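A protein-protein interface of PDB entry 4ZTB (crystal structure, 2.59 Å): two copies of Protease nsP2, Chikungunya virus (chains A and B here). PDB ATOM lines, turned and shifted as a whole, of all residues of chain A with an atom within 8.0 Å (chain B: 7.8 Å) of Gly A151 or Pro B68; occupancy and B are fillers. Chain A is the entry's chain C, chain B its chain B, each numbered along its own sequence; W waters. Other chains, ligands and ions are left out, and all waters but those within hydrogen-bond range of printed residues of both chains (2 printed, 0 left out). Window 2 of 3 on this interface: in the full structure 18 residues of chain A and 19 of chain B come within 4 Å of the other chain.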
ATOM      1  N   PRO A 148       1.917   7.059 -21.873  1.00  0.00           N
ATOM      2  CA  PRO A 148       0.576   7.702 -21.935  1.00  0.00           C
ATOM      3  C   PRO A 148      -0.116   7.806 -20.550  1.00  0.00           C
ATOM      4  O   PRO A 148       0.259   7.069 -19.630  1.00  0.00           O
ATOM      5  CB  PRO A 148      -0.216   6.779 -22.880  1.00  0.00           C
ATOM      6  CG  PRO A 148       0.819   6.022 -23.645  1.00  0.00           C
ATOM      7  CD  PRO A 148       1.948   5.819 -22.677  1.00  0.00           C
ATOM      8  N   VAL A 149      -1.094   8.713 -20.418  1.00  0.00           N
ATOM      9  CA  VAL A 149      -1.820   8.930 -19.179  1.00  0.00           C
ATOM     10  C   VAL A 149      -3.305   9.012 -19.503  1.00  0.00           C
ATOM     11  O   VAL A 149      -3.704   9.898 -20.274  1.00  0.00           O
ATOM     12  CB  VAL A 149      -1.397  10.273 -18.459  1.00  0.00           C
ATOM     13  CG1 VAL A 149      -2.210  10.508 -17.169  1.00  0.00           C
ATOM     14  CG2 VAL A 149       0.100  10.351 -18.169  1.00  0.00           C
ATOM     15  N   LYS A 150      -4.107   8.097 -18.928  1.00  0.00           N
ATOM     16  CA  LYS A 150      -5.559   8.119 -19.046  1.00  0.00           C
ATOM     17  C   LYS A 150      -6.020   9.201 -18.074  1.00  0.00           C
ATOM     18  O   LYS A 150      -6.312   8.921 -16.906  1.00  0.00           O
ATOM     19  CB  LYS A 150      -6.200   6.766 -18.700  1.00  0.00           C
ATOM     20  CG  LYS A 150      -5.904   5.620 -19.635  1.00  0.00           C
ATOM     21  CD  LYS A 150      -6.431   4.294 -19.071  1.00  0.00           C
ATOM     22  CE  LYS A 150      -6.326   3.157 -20.078  1.00  0.00           C
ATOM     23  NZ  LYS A 150      -4.916   2.813 -20.419  1.00  0.00           N
ATOM     24  N   GLY A 151      -6.071  10.437 -18.574  1.00  0.00           N
ATOM     25  CA  GLY A 151      -6.400  11.615 -17.776  1.00  0.00           C
ATOM     26  C   GLY A 151      -7.826  12.118 -17.828  1.00  0.00           C
ATOM     27  O   GLY A 151      -8.749  11.450 -18.309  1.00  0.00           O
ATOM     28  N   GLU A 152      -7.977  13.316 -17.288  1.00  0.00           N
ATOM     29  CA  GLU A 152      -9.223  14.074 -17.283  1.00  0.00           C
ATOM     30  C   GLU A 152      -9.484  14.773 -18.584  1.00  0.00           C
ATOM     31  O   GLU A 152      -8.611  14.838 -19.435  1.00  0.00           O
ATOM     32  CB  GLU A 152      -9.193  15.143 -16.140  1.00  0.00           C
ATOM     33  CG  GLU A 152      -9.339  14.344 -14.849  1.00  0.00           C
ATOM     34  CD  GLU A 152     -10.777  14.009 -14.574  1.00  0.00           C
ATOM     35  OE1 GLU A 152     -11.647  14.546 -15.297  1.00  0.00           O
ATOM     36  OE2 GLU A 152     -11.027  13.216 -13.664  1.00  0.00           O
ATOM     37  N   ARG A 153     -10.700  15.292 -18.729  1.00  0.00           N
ATOM     38  CA  ARG A 153     -11.048  16.120 -19.878  1.00  0.00           C
ATOM     39  C   ARG A 153     -10.410  17.505 -19.707  1.00  0.00           C
ATOM     40  O   ARG A 153     -10.329  18.035 -18.590  1.00  0.00           O
ATOM     41  CB  ARG A 153     -12.550  16.280 -20.012  1.00  0.00           C
ATOM     42  CG  ARG A 153     -13.349  14.986 -20.173  1.00  0.00           C
ATOM     43  CD  ARG A 153     -14.842  15.283 -20.141  1.00  0.00           C
ATOM     44  NE  ARG A 153     -15.231  16.186 -21.235  1.00  0.00           N
ATOM     45  CZ  ARG A 153     -16.450  16.702 -21.425  1.00  0.00           C
ATOM     46  NH1 ARG A 153     -17.475  16.422 -20.593  1.00  0.00           N
ATOM     47  NH2 ARG A 153     -16.657  17.514 -22.468  1.00  0.00           N
ATOM     48  N   MET A 154      -9.958  18.079 -20.822  1.00  0.00           N
ATOM     49  CA  MET A 154      -9.327  19.437 -20.839  1.00  0.00           C
ATOM     50  C   MET A 154     -10.284  20.571 -20.474  1.00  0.00           C
ATOM     51  O   MET A 154      -9.852  21.591 -19.925  1.00  0.00           O
ATOM     52  CB  MET A 154      -8.717  19.688 -22.197  1.00  0.00           C
ATOM     53  CG  MET A 154      -8.252  21.109 -22.500  1.00  0.00           C
ATOM     54  SD  MET A 154      -7.215  21.186 -23.954  1.00  0.00           S
ATOM     55  CE  MET A 154      -8.022  19.968 -24.988  1.00  0.00           C
ATOM     56  N   GLU A 155     -11.567  20.380 -20.774  1.00  0.00           N
ATOM     57  CA  GLU A 155     -12.640  21.341 -20.461  1.00  0.00           C
ATOM     58  C   GLU A 155     -12.575  21.801 -18.978  1.00  0.00           C
ATOM     59  O   GLU A 155     -12.816  22.962 -18.676  1.00  0.00           O
ATOM     60  CB  GLU A 155     -14.023  20.754 -20.807  1.00  0.00           C
ATOM     61  CG  GLU A 155     -14.376  20.629 -22.305  1.00  0.00           C
ATOM     62  CD  GLU A 155     -13.734  19.466 -23.067  1.00  0.00           C
ATOM     63  OE1 GLU A 155     -12.659  18.977 -22.681  1.00  0.00           O
ATOM     64  OE2 GLU A 155     -14.323  19.044 -24.070  1.00  0.00           O
ATOM     65  N   PRO A 283      -1.707  19.694 -15.054  1.00  0.00           N
ATOM     66  CA  PRO A 283      -2.964  19.292 -14.459  1.00  0.00           C
ATOM     67  C   PRO A 283      -3.360  17.848 -14.805  1.00  0.00           C
ATOM     68  O   PRO A 283      -2.725  17.230 -15.647  1.00  0.00           O
ATOM     69  CB  PRO A 283      -3.956  20.264 -15.089  1.00  0.00           C
ATOM     70  CG  PRO A 283      -3.414  20.464 -16.456  1.00  0.00           C
ATOM     71  CD  PRO A 283      -1.920  20.426 -16.321  1.00  0.00           C
ATOM     72  N   PRO A 284      -4.411  17.313 -14.143  1.00  0.00           N
ATOM     73  CA  PRO A 284      -4.980  15.984 -14.463  1.00  0.00           C
ATOM     74  C   PRO A 284      -5.438  15.753 -15.918  1.00  0.00           C
ATOM     75  O   PRO A 284      -5.559  14.586 -16.307  1.00  0.00           O
ATOM     76  CB  PRO A 284      -6.211  15.896 -13.541  1.00  0.00           C
ATOM     77  CG  PRO A 284      -5.867  16.750 -12.378  1.00  0.00           C
ATOM     78  CD  PRO A 284      -5.009  17.868 -12.908  1.00  0.00           C
ATOM     79  N   CYS A 285      -5.690  16.817 -16.703  1.00  0.00           N
ATOM     80  CA  CYS A 285      -6.169  16.671 -18.097  1.00  0.00           C
ATOM     81  C   CYS A 285      -5.074  16.461 -19.199  1.00  0.00           C
ATOM     82  O   CYS A 285      -5.332  16.711 -20.395  1.00  0.00           O
ATOM     83  CB  CYS A 285      -7.056  17.868 -18.455  1.00  0.00           C
ATOM     84  SG  CYS A 285      -6.144  19.403 -18.553  1.00  0.00           S
ATOM     85  N   VAL A 286      -3.877  16.011 -18.803  1.00  0.00           N
ATOM     86  CA  VAL A 286      -2.797  15.685 -19.758  1.00  0.00           C
ATOM     87  C   VAL A 286      -3.035  14.291 -20.368  1.00  0.00           C
ATOM     88  O   VAL A 286      -3.672  13.424 -19.726  1.00  0.00           O
ATOM     89  CB  VAL A 286      -1.360  15.774 -19.126  1.00  0.00           C
ATOM     90  CG1 VAL A 286      -1.054  17.207 -18.691  1.00  0.00           C
ATOM     91  CG2 VAL A 286      -1.129  14.799 -17.953  1.00  0.00           C
ATOM     92  N   THR A 287      -2.529  14.091 -21.599  1.00  0.00           N
ATOM     93  CA  THR A 287      -2.592  12.791 -22.319  1.00  0.00           C
ATOM     94  C   THR A 287      -1.270  11.974 -22.232  1.00  0.00           C
ATOM     95  O   THR A 287      -1.206  10.840 -22.744  1.00  0.00           O
ATOM     96  CB  THR A 287      -2.970  12.963 -23.808  1.00  0.00           C
ATOM     97  OG1 THR A 287      -1.971  13.740 -24.491  1.00  0.00           O
ATOM     98  CG2 THR A 287      -4.292  13.648 -23.943  1.00  0.00           C
ATOM     99  N   SER A 288      -0.220  12.531 -21.603  1.00  0.00           N
ATOM    100  CA  SER A 288       1.052  11.824 -21.467  1.00  0.00           C
ATOM    101  C   SER A 288       1.953  12.361 -20.343  1.00  0.00           C
ATOM    102  O   SER A 288       1.737  13.438 -19.768  1.00  0.00           O
ATOM    103  CB  SER A 288       1.836  11.868 -22.799  1.00  0.00           C
ATOM    104  OG  SER A 288       2.448  13.132 -23.016  1.00  0.00           O
ATOM    105  N   PHE B  65     -19.733   8.607 -23.502  1.00  0.00           N
ATOM    106  CA  PHE B  65     -18.458   8.403 -24.213  1.00  0.00           C
ATOM    107  C   PHE B  65     -17.457   9.586 -24.059  1.00  0.00           C
ATOM    108  O   PHE B  65     -16.540   9.737 -24.881  1.00  0.00           O
ATOM    109  CB  PHE B  65     -18.754   8.091 -25.691  1.00  0.00           C
ATOM    110  CG  PHE B  65     -19.349   6.720 -25.910  1.00  0.00           C
ATOM    111  CD1 PHE B  65     -18.521   5.580 -25.902  1.00  0.00           C
ATOM    112  CD2 PHE B  65     -20.720   6.552 -26.127  1.00  0.00           C
ATOM    113  CE1 PHE B  65     -19.049   4.311 -26.103  1.00  0.00           C
ATOM    114  CE2 PHE B  65     -21.257   5.277 -26.332  1.00  0.00           C
ATOM    115  CZ  PHE B  65     -20.417   4.155 -26.319  1.00  0.00           C
ATOM    116  N   SER B  66     -17.606  10.400 -23.003  1.00  0.00           N
ATOM    117  CA  SER B  66     -16.760  11.623 -22.805  1.00  0.00           C
ATOM    118  C   SER B  66     -15.428  11.448 -22.031  1.00  0.00           C
ATOM    119  O   SER B  66     -14.675  12.424 -21.907  1.00  0.00           O
ATOM    120  CB  SER B  66     -17.593  12.724 -22.126  1.00  0.00           C
ATOM    121  OG  SER B  66     -17.962  12.355 -20.815  1.00  0.00           O
ATOM    122  N   LYS B  67     -15.137  10.243 -21.517  1.00  0.00           N
ATOM    123  CA  LYS B  67     -13.890  10.001 -20.797  1.00  0.00           C
ATOM    124  C   LYS B  67     -12.814   9.830 -21.875  1.00  0.00           C
ATOM    125  O   LYS B  67     -12.945   8.933 -22.710  1.00  0.00           O
ATOM    126  CB  LYS B  67     -13.973   8.768 -19.891  1.00  0.00           C
ATOM    127  CG  LYS B  67     -12.773   8.593 -18.940  1.00  0.00           C
ATOM    128  CD  LYS B  67     -12.789   7.230 -18.252  1.00  0.00           C
ATOM    129  CE  LYS B  67     -11.514   6.961 -17.450  1.00  0.00           C
ATOM    130  NZ  LYS B  67     -11.402   7.769 -16.216  1.00  0.00           N
ATOM    131  N   PRO B  68     -11.749  10.680 -21.866  1.00  0.00           N
ATOM    132  CA  PRO B  68     -10.741  10.587 -22.925  1.00  0.00           C
ATOM    133  C   PRO B  68      -9.837   9.369 -22.739  1.00  0.00           C
ATOM    134  O   PRO B  68      -8.792   9.445 -22.086  1.00  0.00           O
ATOM    135  CB  PRO B  68      -9.983  11.922 -22.804  1.00  0.00           C
ATOM    136  CG  PRO B  68     -10.072  12.259 -21.374  1.00  0.00           C
ATOM    137  CD  PRO B  68     -11.393  11.729 -20.884  1.00  0.00           C
ATOM    138  N   LEU B  69     -10.274   8.252 -23.320  1.00  0.00           N
ATOM    139  CA  LEU B  69      -9.532   6.981 -23.307  1.00  0.00           C
ATOM    140  C   LEU B  69      -8.835   6.677 -24.632  1.00  0.00           C
ATOM    141  O   LEU B  69      -7.658   6.307 -24.638  1.00  0.00           O
ATOM    142  CB  LEU B  69     -10.474   5.818 -22.975  1.00  0.00           C
ATOM    143  CG  LEU B  69     -11.149   5.779 -21.597  1.00  0.00           C
ATOM    144  CD1 LEU B  69     -12.069   4.578 -21.495  1.00  0.00           C
ATOM    145  CD2 LEU B  69     -10.116   5.724 -20.493  1.00  0.00           C
ATOM    146  N   VAL B  70      -9.565   6.834 -25.742  1.00  0.00           N
ATOM    147  CA  VAL B  70      -9.101   6.466 -27.081  1.00  0.00           C
ATOM    148  C   VAL B  70      -9.262   7.608 -28.075  1.00  0.00           C
ATOM    149  O   VAL B  70     -10.362   8.142 -28.219  1.00  0.00           O
ATOM    150  CB  VAL B  70      -9.920   5.240 -27.579  1.00  0.00           C
ATOM    151  CG1 VAL B  70      -9.595   4.865 -29.018  1.00  0.00           C
ATOM    152  CG2 VAL B  70      -9.704   4.034 -26.654  1.00  0.00           C
ATOM    153  N   SER B  71      -8.171   7.949 -28.769  1.00  0.00           N
ATOM    154  CA  SER B  71      -8.144   9.006 -29.791  1.00  0.00           C
ATOM    155  C   SER B  71      -8.576   8.527 -31.174  1.00  0.00           C
ATOM    156  O   SER B  71      -8.391   7.352 -31.520  1.00  0.00           O
ATOM    157  CB  SER B  71      -6.730   9.571 -29.912  1.00  0.00           C
ATOM    158  OG  SER B  71      -6.640  10.572 -30.913  1.00  0.00           O
ATOM    159  N   GLY B  85      -5.657  13.300 -31.398  1.00  0.00           N
ATOM    160  CA  GLY B  85      -6.982  13.580 -31.979  1.00  0.00           C
ATOM    161  C   GLY B  85      -8.000  13.702 -30.868  1.00  0.00           C
ATOM    162  O   GLY B  85      -7.633  13.666 -29.680  1.00  0.00           O
ATOM    163  N   LYS B  86      -9.278  13.855 -31.239  1.00  0.00           N
ATOM    164  CA  LYS B  86     -10.361  13.949 -30.245  1.00  0.00           C
ATOM    165  C   LYS B  86     -10.483  12.604 -29.576  1.00  0.00           C
ATOM    166  O   LYS B  86     -10.461  11.583 -30.257  1.00  0.00           O
ATOM    167  CB  LYS B  86     -11.684  14.341 -30.881  1.00  0.00           C
ATOM    168  CG  LYS B  86     -12.737  14.758 -29.864  1.00  0.00           C
ATOM    169  CD  LYS B  86     -13.944  15.391 -30.545  1.00  0.00           C
ATOM    170  CE  LYS B  86     -15.090  15.684 -29.570  1.00  0.00           C
ATOM    171  NZ  LYS B  86     -14.716  16.599 -28.447  1.00  0.00           N
ATOM    172  N   MET B  87     -10.607  12.596 -28.254  1.00  0.00           N
ATOM    173  CA  MET B  87     -10.638  11.349 -27.478  1.00  0.00           C
ATOM    174  C   MET B  87     -12.018  11.032 -26.915  1.00  0.00           C
ATOM    175  O   MET B  87     -12.709  11.931 -26.440  1.00  0.00           O
ATOM    176  CB  MET B  87      -9.603  11.421 -26.358  1.00  0.00           C
ATOM    177  CG  MET B  87      -8.184  11.532 -26.905  1.00  0.00           C
ATOM    178  SD  MET B  87      -6.870  11.458 -25.697  1.00  0.00           S
ATOM    179  CE  MET B  87      -6.973   9.744 -25.167  1.00  0.00           C
ATOM    180  N   PHE B  88     -12.397   9.744 -26.992  1.00  0.00           N
ATOM    181  CA  PHE B  88     -13.662   9.213 -26.467  1.00  0.00           C
ATOM    182  C   PHE B  88     -13.376   7.980 -25.609  1.00  0.00           C
ATOM    183  O   PHE B  88     -12.242   7.477 -25.562  1.00  0.00           O
ATOM    184  CB  PHE B  88     -14.634   8.824 -27.592  1.00  0.00           C
ATOM    185  CG  PHE B  88     -15.010   9.955 -28.515  1.00  0.00           C
ATOM    186  CD1 PHE B  88     -16.053  10.844 -28.183  1.00  0.00           C
ATOM    187  CD2 PHE B  88     -14.339  10.135 -29.730  1.00  0.00           C
ATOM    188  CE1 PHE B  88     -16.401  11.891 -29.046  1.00  0.00           C
ATOM    189  CE2 PHE B  88     -14.683  11.175 -30.595  1.00  0.00           C
ATOM    190  CZ  PHE B  88     -15.713  12.053 -30.251  1.00  0.00           C
ATOM    191  N   GLY B  89     -14.413   7.497 -24.932  1.00  0.00           N
ATOM    192  CA  GLY B  89     -14.331   6.298 -24.076  1.00  0.00           C
ATOM    193  C   GLY B  89     -15.420   6.294 -23.025  1.00  0.00           C
ATOM    194  O   GLY B  89     -15.843   7.369 -22.588  1.00  0.00           O
ATOM    195  N   PHE B  90     -15.866   5.101 -22.611  1.00  0.00           N
ATOM    196  CA  PHE B  90     -16.958   4.979 -21.616  1.00  0.00           C
ATOM    197  C   PHE B  90     -16.623   5.734 -20.327  1.00  0.00           C
ATOM    198  O   PHE B  90     -15.512   5.603 -19.818  1.00  0.00           O
ATOM    199  CB  PHE B  90     -17.301   3.526 -21.284  1.00  0.00           C
ATOM    200  CG  PHE B  90     -18.586   3.377 -20.500  1.00  0.00           C
ATOM    201  CD1 PHE B  90     -19.832   3.422 -21.150  1.00  0.00           C
ATOM    202  CD2 PHE B  90     -18.565   3.199 -19.099  1.00  0.00           C
ATOM    203  CE1 PHE B  90     -21.033   3.289 -20.428  1.00  0.00           C
ATOM    204  CE2 PHE B  90     -19.767   3.066 -18.370  1.00  0.00           C
ATOM    205  CZ  PHE B  90     -21.002   3.111 -19.042  1.00  0.00           C
ATOM    206  N   ASN B  91     -17.594   6.512 -19.830  1.00  0.00           N
ATOM    207  CA  ASN B  91     -17.456   7.337 -18.639  1.00  0.00           C
ATOM    208  C   ASN B  91     -18.422   6.869 -17.548  1.00  0.00           C
ATOM    209  O   ASN B  91     -19.616   7.208 -17.606  1.00  0.00           O
ATOM    210  CB  ASN B  91     -17.706   8.803 -19.010  1.00  0.00           C
ATOM    211  CG  ASN B  91     -17.448   9.782 -17.856  1.00  0.00           C
ATOM    212  OD1 ASN B  91     -16.796   9.463 -16.853  1.00  0.00           O
ATOM    213  ND2 ASN B  91     -17.963  10.995 -18.009  1.00  0.00           N
HETATM  214  O   HOH W   1     -11.698  11.115 -16.455  1.00  0.00           O
HETATM  215  O   HOH W   2      -8.954   8.716 -19.199  1.00  0.00           O
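Of the 14 printed residues of chain B, 3 touch a printed residue of chain A. Hydrophobic or aromatic side chains of chain B within 4 Å of the printed part of chain A: Pro B68 and Met B87.
Gly A151 touches just one residue of chain B: Pro B68. Of the printed residues of chain B, Arg A153 touches Ser B66 (3.4 Å) and Pro B68 (3.9 Å). Of the printed residues of chain B, Thr A287 touches Met B87. Pro B68 touches three residues of chain A. Ser B71 touches none of the printed residues of chain A. Printed residues of chain A within 4 Å of Met B87: Thr A287 (3.8 Å). Phe B88 touches none of the printed residues of chain A. The nearest residue of chain A that does not touch Pro B68 is Lys A150 (4.6 Å).
Water W2 bridges O of Gly A151 (2.9 Å) and O of Pro B68 (3.0 Å). Water W1 bridges the side-chain amino group (NZ) of Lys B67 (3.4 Å) and the backbone carbonyl oxygen (O) of Gly A151 (3.5 Å).
The guanidinium group (NH2) of Arg A153 lies within salt-bridge range of the side-chain carboxylate (OE2) of Glu A155 (3.2 Å). The backbone NH (N) of Val A149 lies within hydrogen-bond range of the backbone carbonyl oxygen (O) of Thr A287 (3.2 Å). O of Pro A284 is in hydrogen-bond range of N of Glu A152, 2.9 Å away. The side-chain amide nitrogen (ND2) of Asn B91 is in hydrogen-bond range of the side-chain hydroxyl (OG) of Ser B66 (3.1 Å).
No position is printed for both chains. Of the 5 pairs that touch across the chains among the printed residues, none has its exchanged pair printed and touching as well.
Gly A151 touches Pro B68. Pro B68 touches Glu A152 (CG to O, 3.5 Å). Ser B66 touches Arg A153. CG of Arg A153 touches CD of Pro B68, at 3.9 Å. Met B87 touches Thr A287.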
